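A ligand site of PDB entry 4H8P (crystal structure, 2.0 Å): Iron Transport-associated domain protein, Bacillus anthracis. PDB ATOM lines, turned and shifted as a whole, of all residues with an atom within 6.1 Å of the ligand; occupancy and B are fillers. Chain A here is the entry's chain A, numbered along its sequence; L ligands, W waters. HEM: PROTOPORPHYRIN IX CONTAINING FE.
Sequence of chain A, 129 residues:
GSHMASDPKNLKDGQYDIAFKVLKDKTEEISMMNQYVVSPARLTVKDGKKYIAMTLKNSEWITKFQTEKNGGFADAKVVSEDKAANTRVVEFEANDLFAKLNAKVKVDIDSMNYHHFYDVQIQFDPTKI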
ATOM      1  N   LEU A  23       6.543 -32.193 -19.248  1.00  0.00           N
ATOM      2  CA  LEU A  23       5.165 -32.568 -19.584  1.00  0.00           C
ATOM      3  C   LEU A  23       4.269 -32.646 -18.366  1.00  0.00           C
ATOM      4  O   LEU A  23       4.688 -33.113 -17.307  1.00  0.00           O
ATOM      5  CB  LEU A  23       5.137 -33.933 -20.272  1.00  0.00           C
ATOM      6  CG  LEU A  23       6.014 -34.092 -21.499  1.00  0.00           C
ATOM      7  CD1 LEU A  23       5.974 -35.544 -21.976  1.00  0.00           C
ATOM      8  CD2 LEU A  23       5.577 -33.114 -22.594  1.00  0.00           C
ATOM      9  N   LYS A  24       3.023 -32.242 -18.527  1.00  0.00           N
ATOM     10  CA  LYS A  24       2.043 -32.328 -17.463  1.00  0.00           C
ATOM     11  C   LYS A  24       1.842 -33.793 -17.084  1.00  0.00           C
ATOM     12  O   LYS A  24       1.812 -34.657 -17.957  1.00  0.00           O
ATOM     13  CB  LYS A  24       0.725 -31.697 -17.941  1.00  0.00           C
ATOM     14  CG  LYS A  24      -0.439 -31.859 -16.984  1.00  0.00           C
ATOM     15  CD  LYS A  24      -1.697 -31.177 -17.546  1.00  0.00           C
ATOM     16  CE  LYS A  24      -2.879 -31.364 -16.591  1.00  0.00           C
ATOM     17  NZ  LYS A  24      -4.069 -30.583 -17.013  1.00  0.00           N
ATOM     18  N   ASP A  25       1.709 -34.073 -15.795  1.00  0.00           N
ATOM     19  CA  ASP A  25       1.746 -35.444 -15.288  1.00  0.00           C
ATOM     20  C   ASP A  25       0.836 -36.397 -16.085  1.00  0.00           C
ATOM     21  O   ASP A  25      -0.346 -36.131 -16.237  1.00  0.00           O
ATOM     22  CB  ASP A  25       1.372 -35.482 -13.802  1.00  0.00           C
ATOM     23  CG  ASP A  25       1.536 -36.871 -13.193  1.00  0.00           C
ATOM     24  OD1 ASP A  25       2.488 -37.590 -13.584  1.00  0.00           O
ATOM     25  OD2 ASP A  25       0.735 -37.218 -12.296  1.00  0.00           O
ATOM     26  N   ILE A  30       2.347 -29.988 -22.822  1.00  0.00           N
ATOM     27  CA  ILE A  30       3.411 -29.169 -22.234  1.00  0.00           C
ATOM     28  C   ILE A  30       3.018 -28.637 -20.865  1.00  0.00           C
ATOM     29  O   ILE A  30       1.965 -27.992 -20.728  1.00  0.00           O
ATOM     30  CB  ILE A  30       3.781 -27.983 -23.143  1.00  0.00           C
ATOM     31  CG1 ILE A  30       4.151 -28.482 -24.536  1.00  0.00           C
ATOM     32  CG2 ILE A  30       4.942 -27.177 -22.542  1.00  0.00           C
ATOM     33  CD1 ILE A  30       5.282 -29.505 -24.524  1.00  0.00           C
ATOM     34  N   SER A  31       3.841 -28.903 -19.852  1.00  0.00           N
ATOM     35  CA  SER A  31       3.573 -28.429 -18.487  1.00  0.00           C
ATOM     36  C   SER A  31       3.772 -26.926 -18.342  1.00  0.00           C
ATOM     37  O   SER A  31       4.562 -26.334 -19.076  1.00  0.00           O
ATOM     38  CB  SER A  31       4.495 -29.162 -17.487  1.00  0.00           C
ATOM     39  OG  SER A  31       4.359 -28.659 -16.164  1.00  0.00           O
ATOM     40  N   MET A  32       3.082 -26.289 -17.387  1.00  0.00           N
ATOM     41  CA  MET A  32       3.346 -24.894 -17.036  1.00  0.00           C
ATOM     42  C   MET A  32       4.813 -24.734 -16.639  1.00  0.00           C
ATOM     43  O   MET A  32       5.418 -23.672 -16.840  1.00  0.00           O
ATOM     44  CB  MET A  32       2.484 -24.439 -15.843  1.00  0.00           C
ATOM     45  CG  MET A  32       0.974 -24.327 -16.111  1.00  0.00           C
ATOM     46  SD  MET A  32       0.550 -22.989 -17.248  1.00  0.00           S
ATOM     47  CE  MET A  32       1.539 -21.638 -16.596  1.00  0.00           C
ATOM     48  N   MET A  33       5.384 -25.786 -16.067  1.00  0.00           N
ATOM     49  CA  MET A  33       6.775 -25.738 -15.605  1.00  0.00           C
ATOM     50  C   MET A  33       7.762 -25.548 -16.745  1.00  0.00           C
ATOM     51  O   MET A  33       8.874 -25.045 -16.537  1.00  0.00           O
ATOM     52  CB  MET A  33       7.131 -27.004 -14.803  1.00  0.00           C
ATOM     53  CG  MET A  33       8.588 -27.068 -14.356  1.00  0.00           C
ATOM     54  SD  MET A  33       8.912 -28.422 -13.185  1.00  0.00           S
ATOM     55  CE  MET A  33      10.649 -28.112 -12.813  1.00  0.00           C
ATOM     56  N   TYR A  36       9.645 -22.504 -17.121  1.00  0.00           N
ATOM     57  CA  TYR A  36      10.608 -22.147 -16.070  1.00  0.00           C
ATOM     58  C   TYR A  36      11.894 -22.971 -16.074  1.00  0.00           C
ATOM     59  O   TYR A  36      12.619 -23.010 -15.067  1.00  0.00           O
ATOM     60  CB  TYR A  36       9.909 -22.216 -14.697  1.00  0.00           C
ATOM     61  CG  TYR A  36       8.767 -21.235 -14.583  1.00  0.00           C
ATOM     62  CD1 TYR A  36       9.007 -19.906 -14.284  1.00  0.00           C
ATOM     63  CD2 TYR A  36       7.454 -21.647 -14.787  1.00  0.00           C
ATOM     64  CE1 TYR A  36       7.957 -18.994 -14.189  1.00  0.00           C
ATOM     65  CE2 TYR A  36       6.398 -20.743 -14.694  1.00  0.00           C
ATOM     66  CZ  TYR A  36       6.661 -19.419 -14.395  1.00  0.00           C
ATOM     67  OH  TYR A  36       5.629 -18.521 -14.301  1.00  0.00           O
ATOM     68  N   LYS A  57      14.606 -21.318 -13.986  1.00  0.00           N
ATOM     69  CA  LYS A  57      14.299 -19.888 -13.909  1.00  0.00           C
ATOM     70  C   LYS A  57      13.352 -19.591 -12.759  1.00  0.00           C
ATOM     71  O   LYS A  57      12.693 -20.502 -12.243  1.00  0.00           O
ATOM     72  CB  LYS A  57      13.664 -19.431 -15.231  1.00  0.00           C
ATOM     73  CG  LYS A  57      14.673 -19.358 -16.381  1.00  0.00           C
ATOM     74  CD  LYS A  57      14.145 -19.976 -17.656  1.00  0.00           C
ATOM     75  CE  LYS A  57      13.183 -19.075 -18.376  1.00  0.00           C
ATOM     76  NZ  LYS A  57      12.922 -19.584 -19.760  1.00  0.00           N
ATOM     77  N   ASN A  58      13.275 -18.332 -12.360  1.00  0.00           N
ATOM     78  CA  ASN A  58      12.499 -17.916 -11.184  1.00  0.00           C
ATOM     79  C   ASN A  58      12.838 -18.802 -10.000  1.00  0.00           C
ATOM     80  O   ASN A  58      11.950 -19.326  -9.314  1.00  0.00           O
ATOM     81  CB  ASN A  58      10.988 -17.953 -11.466  1.00  0.00           C
ATOM     82  CG  ASN A  58      10.535 -16.806 -12.370  1.00  0.00           C
ATOM     83  OD1 ASN A  58      10.539 -16.914 -13.593  1.00  0.00           O
ATOM     84  ND2 ASN A  58      10.166 -15.697 -11.753  1.00  0.00           N
ATOM     85  N   TRP A  61      11.134 -19.019  -6.504  1.00  0.00           N
ATOM     86  CA  TRP A  61       9.807 -19.649  -6.446  1.00  0.00           C
ATOM     87  C   TRP A  61       9.798 -21.184  -6.346  1.00  0.00           C
ATOM     88  O   TRP A  61       8.857 -21.779  -5.806  1.00  0.00           O
ATOM     89  CB  TRP A  61       9.023 -19.275  -7.695  1.00  0.00           C
ATOM     90  CG  TRP A  61       8.597 -17.839  -7.776  1.00  0.00           C
ATOM     91  CD1 TRP A  61       8.717 -16.889  -6.799  1.00  0.00           C
ATOM     92  CD2 TRP A  61       7.959 -17.211  -8.888  1.00  0.00           C
ATOM     93  NE1 TRP A  61       8.198 -15.698  -7.254  1.00  0.00           N
ATOM     94  CE2 TRP A  61       7.722 -15.863  -8.526  1.00  0.00           C
ATOM     95  CE3 TRP A  61       7.558 -17.648 -10.163  1.00  0.00           C
ATOM     96  CZ2 TRP A  61       7.106 -14.948  -9.390  1.00  0.00           C
ATOM     97  CZ3 TRP A  61       6.952 -16.742 -11.023  1.00  0.00           C
ATOM     98  CH2 TRP A  61       6.729 -15.407 -10.627  1.00  0.00           C
ATOM     99  N   ILE A  62      10.826 -21.818  -6.895  1.00  0.00           N
ATOM    100  CA  ILE A  62      10.864 -23.269  -6.975  1.00  0.00           C
ATOM    101  C   ILE A  62      11.580 -23.754  -5.732  1.00  0.00           C
ATOM    102  O   ILE A  62      12.806 -23.667  -5.649  1.00  0.00           O
ATOM    103  CB  ILE A  62      11.582 -23.743  -8.256  1.00  0.00           C
ATOM    104  CG1 ILE A  62      10.873 -23.176  -9.491  1.00  0.00           C
ATOM    105  CG2 ILE A  62      11.625 -25.278  -8.304  1.00  0.00           C
ATOM    106  CD1 ILE A  62      11.584 -23.412 -10.821  1.00  0.00           C
ATOM    107  N   VAL A 105       7.968 -31.207  -8.201  1.00  0.00           N
ATOM    108  CA  VAL A 105       8.365 -29.828  -7.968  1.00  0.00           C
ATOM    109  C   VAL A 105       7.434 -29.187  -6.960  1.00  0.00           C
ATOM    110  O   VAL A 105       6.225 -29.477  -6.914  1.00  0.00           O
ATOM    111  CB  VAL A 105       8.405 -29.018  -9.278  1.00  0.00           C
ATOM    112  CG1 VAL A 105       7.002 -28.842  -9.863  1.00  0.00           C
ATOM    113  CG2 VAL A 105       9.061 -27.660  -9.055  1.00  0.00           C
ATOM    114  N   VAL A 107       6.367 -25.378  -5.460  1.00  0.00           N
ATOM    115  CA  VAL A 107       6.403 -23.974  -5.856  1.00  0.00           C
ATOM    116  C   VAL A 107       5.787 -23.144  -4.747  1.00  0.00           C
ATOM    117  O   VAL A 107       4.765 -23.517  -4.164  1.00  0.00           O
ATOM    118  CB  VAL A 107       5.648 -23.756  -7.169  1.00  0.00           C
ATOM    119  CG1 VAL A 107       5.774 -22.299  -7.649  1.00  0.00           C
ATOM    120  CG2 VAL A 107       6.146 -24.715  -8.237  1.00  0.00           C
ATOM    121  N   ILE A 109       4.949 -19.007  -3.978  1.00  0.00           N
ATOM    122  CA  ILE A 109       4.960 -17.571  -4.258  1.00  0.00           C
ATOM    123  C   ILE A 109       4.112 -16.884  -3.218  1.00  0.00           C
ATOM    124  O   ILE A 109       2.874 -16.846  -3.303  1.00  0.00           O
ATOM    125  CB  ILE A 109       4.431 -17.263  -5.661  1.00  0.00           C
ATOM    126  CG1 ILE A 109       5.044 -18.214  -6.692  1.00  0.00           C
ATOM    127  CG2 ILE A 109       4.761 -15.822  -6.033  1.00  0.00           C
ATOM    128  CD1 ILE A 109       4.610 -17.929  -8.096  1.00  0.00           C
ATOM    129  N   MET A 112       1.538 -13.986  -4.174  1.00  0.00           N
ATOM    130  CA  MET A 112       0.395 -14.328  -4.995  1.00  0.00           C
ATOM    131  C   MET A 112      -0.349 -15.512  -4.385  1.00  0.00           C
ATOM    132  O   MET A 112      -1.183 -16.134  -5.042  1.00  0.00           O
ATOM    133  CB  MET A 112       0.813 -14.657  -6.430  1.00  0.00           C
ATOM    134  CG  MET A 112       1.705 -13.606  -7.097  1.00  0.00           C
ATOM    135  SD  MET A 112       2.388 -14.190  -8.663  1.00  0.00           S
ATOM    136  CE  MET A 112       3.881 -13.175  -8.768  1.00  0.00           C
ATOM    137  N   TYR A 114       0.442 -18.572  -3.918  1.00  0.00           N
ATOM    138  CA  TYR A 114       0.515 -19.744  -4.776  1.00  0.00           C
ATOM    139  C   TYR A 114       1.445 -20.752  -4.134  1.00  0.00           C
ATOM    140  O   TYR A 114       2.653 -20.547  -4.076  1.00  0.00           O
ATOM    141  CB  TYR A 114       1.025 -19.353  -6.159  1.00  0.00           C
ATOM    142  CG  TYR A 114       1.095 -20.457  -7.172  1.00  0.00           C
ATOM    143  CD1 TYR A 114      -0.009 -20.796  -7.939  1.00  0.00           C
ATOM    144  CD2 TYR A 114       2.287 -21.150  -7.384  1.00  0.00           C
ATOM    145  CE1 TYR A 114       0.060 -21.804  -8.889  1.00  0.00           C
ATOM    146  CE2 TYR A 114       2.369 -22.155  -8.338  1.00  0.00           C
ATOM    147  CZ  TYR A 114       1.254 -22.488  -9.086  1.00  0.00           C
ATOM    148  OH  TYR A 114       1.348 -23.477 -10.038  1.00  0.00           O
ATOM    149  N   TYR A 118       3.655 -30.621  -7.465  1.00  0.00           N
ATOM    150  CA  TYR A 118       3.133 -31.346  -8.602  1.00  0.00           C
ATOM    151  C   TYR A 118       4.091 -32.448  -9.003  1.00  0.00           C
ATOM    152  O   TYR A 118       5.288 -32.413  -8.687  1.00  0.00           O
ATOM    153  CB  TYR A 118       3.002 -30.428  -9.822  1.00  0.00           C
ATOM    154  CG  TYR A 118       2.218 -29.144  -9.659  1.00  0.00           C
ATOM    155  CD1 TYR A 118       0.828 -29.136  -9.810  1.00  0.00           C
ATOM    156  CD2 TYR A 118       2.868 -27.936  -9.414  1.00  0.00           C
ATOM    157  CE1 TYR A 118       0.108 -27.948  -9.701  1.00  0.00           C
ATOM    158  CE2 TYR A 118       2.148 -26.748  -9.304  1.00  0.00           C
ATOM    159  CZ  TYR A 118       0.767 -26.760  -9.444  1.00  0.00           C
ATOM    160  OH  TYR A 118       0.061 -25.581  -9.344  1.00  0.00           O
ATOM    161  N   ASP A 119       3.548 -33.397  -9.762  1.00  0.00           N
ATOM    162  CA  ASP A 119       4.350 -34.372 -10.475  1.00  0.00           C
ATOM    163  C   ASP A 119       4.434 -33.911 -11.935  1.00  0.00           C
ATOM    164  O   ASP A 119       3.473 -33.360 -12.463  1.00  0.00           O
ATOM    165  CB  ASP A 119       3.646 -35.736 -10.416  1.00  0.00           C
ATOM    166  CG  ASP A 119       3.686 -36.362  -9.016  1.00  0.00           C
ATOM    167  OD1 ASP A 119       2.608 -36.579  -8.428  1.00  0.00           O
ATOM    168  OD2 ASP A 119       4.778 -36.657  -8.517  1.00  0.00           O
ATOM    169  N   VAL A 120       5.578 -34.121 -12.564  1.00  0.00           N
ATOM    170  CA  VAL A 120       5.708 -33.861 -13.999  1.00  0.00           C
ATOM    171  C   VAL A 120       6.586 -34.931 -14.608  1.00  0.00           C
ATOM    172  O   VAL A 120       7.270 -35.657 -13.878  1.00  0.00           O
ATOM    173  CB  VAL A 120       6.329 -32.476 -14.280  1.00  0.00           C
ATOM    174  CG1 VAL A 120       5.425 -31.368 -13.726  1.00  0.00           C
ATOM    175  CG2 VAL A 120       7.738 -32.379 -13.679  1.00  0.00           C
HETATM  176  CHA HEM L   1      -0.512 -25.700 -12.854  1.00  0.00           C
HETATM  177  CHB HEM L   1      -0.746 -20.846 -12.647  1.00  0.00           C
HETATM  178  CHC HEM L   1       3.980 -20.705 -11.555  1.00  0.00           C
HETATM  179  CHD HEM L   1       4.325 -25.435 -12.333  1.00  0.00           C
HETATM  180  C1A HEM L   1      -0.984 -24.411 -12.873  1.00  0.00           C
HETATM  181  C2A HEM L   1      -2.361 -24.027 -13.083  1.00  0.00           C
HETATM  182  C3A HEM L   1      -2.443 -22.691 -13.032  1.00  0.00           C
HETATM  183  C4A HEM L   1      -1.108 -22.174 -12.781  1.00  0.00           C
HETATM  184  CMA HEM L   1      -3.735 -21.845 -13.201  1.00  0.00           C
HETATM  185  CAA HEM L   1      -3.530 -25.015 -13.328  1.00  0.00           C
HETATM  186  CBA HEM L   1      -4.147 -24.672 -14.669  1.00  0.00           C
HETATM  187  CGA HEM L   1      -3.176 -25.030 -15.762  1.00  0.00           C
HETATM  188  O1A HEM L   1      -2.812 -24.127 -16.577  1.00  0.00           O
HETATM  189  O2A HEM L   1      -2.784 -26.227 -15.789  1.00  0.00           O
HETATM  190  C1B HEM L   1       0.509 -20.385 -12.353  1.00  0.00           C
HETATM  191  C2B HEM L   1       0.941 -18.992 -12.267  1.00  0.00           C
HETATM  192  C3B HEM L   1       2.251 -18.991 -11.976  1.00  0.00           C
HETATM  193  C4B HEM L   1       2.687 -20.350 -11.856  1.00  0.00           C
HETATM  194  CMB HEM L   1       0.029 -17.773 -12.506  1.00  0.00           C
HETATM  195  CAB HEM L   1       3.239 -17.825 -11.746  1.00  0.00           C
HETATM  196  CBB HEM L   1       2.786 -16.625 -11.405  1.00  0.00           C
HETATM  197  C1C HEM L   1       4.510 -21.948 -11.680  1.00  0.00           C
HETATM  198  C2C HEM L   1       5.913 -22.311 -11.495  1.00  0.00           C
HETATM  199  C3C HEM L   1       6.009 -23.629 -11.706  1.00  0.00           C
HETATM  200  C4C HEM L   1       4.678 -24.142 -12.037  1.00  0.00           C
HETATM  201  CMC HEM L   1       7.033 -21.325 -11.115  1.00  0.00           C
HETATM  202  CAC HEM L   1       7.314 -24.451 -11.624  1.00  0.00           C
HETATM  203  CBC HEM L   1       7.258 -25.785 -11.653  1.00  0.00           C
HETATM  204  C1D HEM L   1       3.073 -25.945 -12.533  1.00  0.00           C
HETATM  205  C2D HEM L   1       2.795 -27.355 -12.746  1.00  0.00           C
HETATM  206  C3D HEM L   1       1.285 -27.431 -12.906  1.00  0.00           C
HETATM  207  C4D HEM L   1       0.806 -26.075 -12.779  1.00  0.00           C
HETATM  208  CMD HEM L   1       3.784 -28.542 -12.791  1.00  0.00           C
HETATM  209  CAD HEM L   1       0.451 -28.702 -13.150  1.00  0.00           C
HETATM  210  CBD HEM L   1      -0.042 -28.696 -14.599  1.00  0.00           C
HETATM  211  CGD HEM L   1       1.115 -28.703 -15.576  1.00  0.00           C
HETATM  212  O1D HEM L   1       1.073 -27.891 -16.541  1.00  0.00           O
HETATM  213  O2D HEM L   1       2.068 -29.529 -15.412  1.00  0.00           O
HETATM  214  NA  HEM L   1      -0.248 -23.262 -12.687  1.00  0.00           N
HETATM  215  NB  HEM L   1       1.616 -21.187 -12.091  1.00  0.00           N
HETATM  216  NC  HEM L   1       3.818 -23.079 -12.003  1.00  0.00           N
HETATM  217  ND  HEM L   1       1.879 -25.227 -12.553  1.00  0.00           N
HETATM  218 FE   HEM L   1       1.683 -23.235 -11.990  1.00  0.00          FE
HETATM  219  O   HOH W   1       3.308 -19.251 -15.094  1.00  0.00           O
HETATM  220  O   HOH W   2       1.729 -31.968 -13.980  1.00  0.00           O
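Water W2 lies within hydrogen-bond range of O of Asp 119, N of Asp 25 and O2D of the ligand.
Merely in contact with the ligand: Met 33, Tyr 118, Val 120, Lys 24, Val 105, Tyr 36, Val 107, Met 112, Trp 61 and Ile 109. Within 4 Å of the ligand: Lys 24, Ser 31, Met 32, Met 33, Tyr 36, Trp 61, Val 105, Val 107, Ile 109, Met 112, Tyr 114, Tyr 118 and Val 120.
N of Met 32 lies within hydrogen-bond range of O1D of the ligand (2.7 Å). The side-chain hydroxyl (OH) of Tyr 114 binds an iron atom (FE) of the ligand (2.0 Å). OG of Ser 31 lies within hydrogen-bond range of O2D of the ligand, at 2.6 Å.
The backbone NH (N) of Ile 109 sits at hydrogen-bond distance from the backbone carbonyl oxygen (O) of Tyr 114, 2.8 Å away. The backbone NH (N) of Tyr 118 is in hydrogen-bond range of the backbone carbonyl oxygen (O) of Val 105, at 2.9 Å. The side-chain hydroxyl (OH) of Tyr 114 lies close to the side-chain hydroxyl (OH) of Tyr 118, at 2.6 Å. The backbone carbonyl oxygen (O) of Tyr 36 lies within hydrogen-bond range of the backbone NH (N) of Lys 57 (2.8 Å). N of Met 33 lies close to OG of Ser 31.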
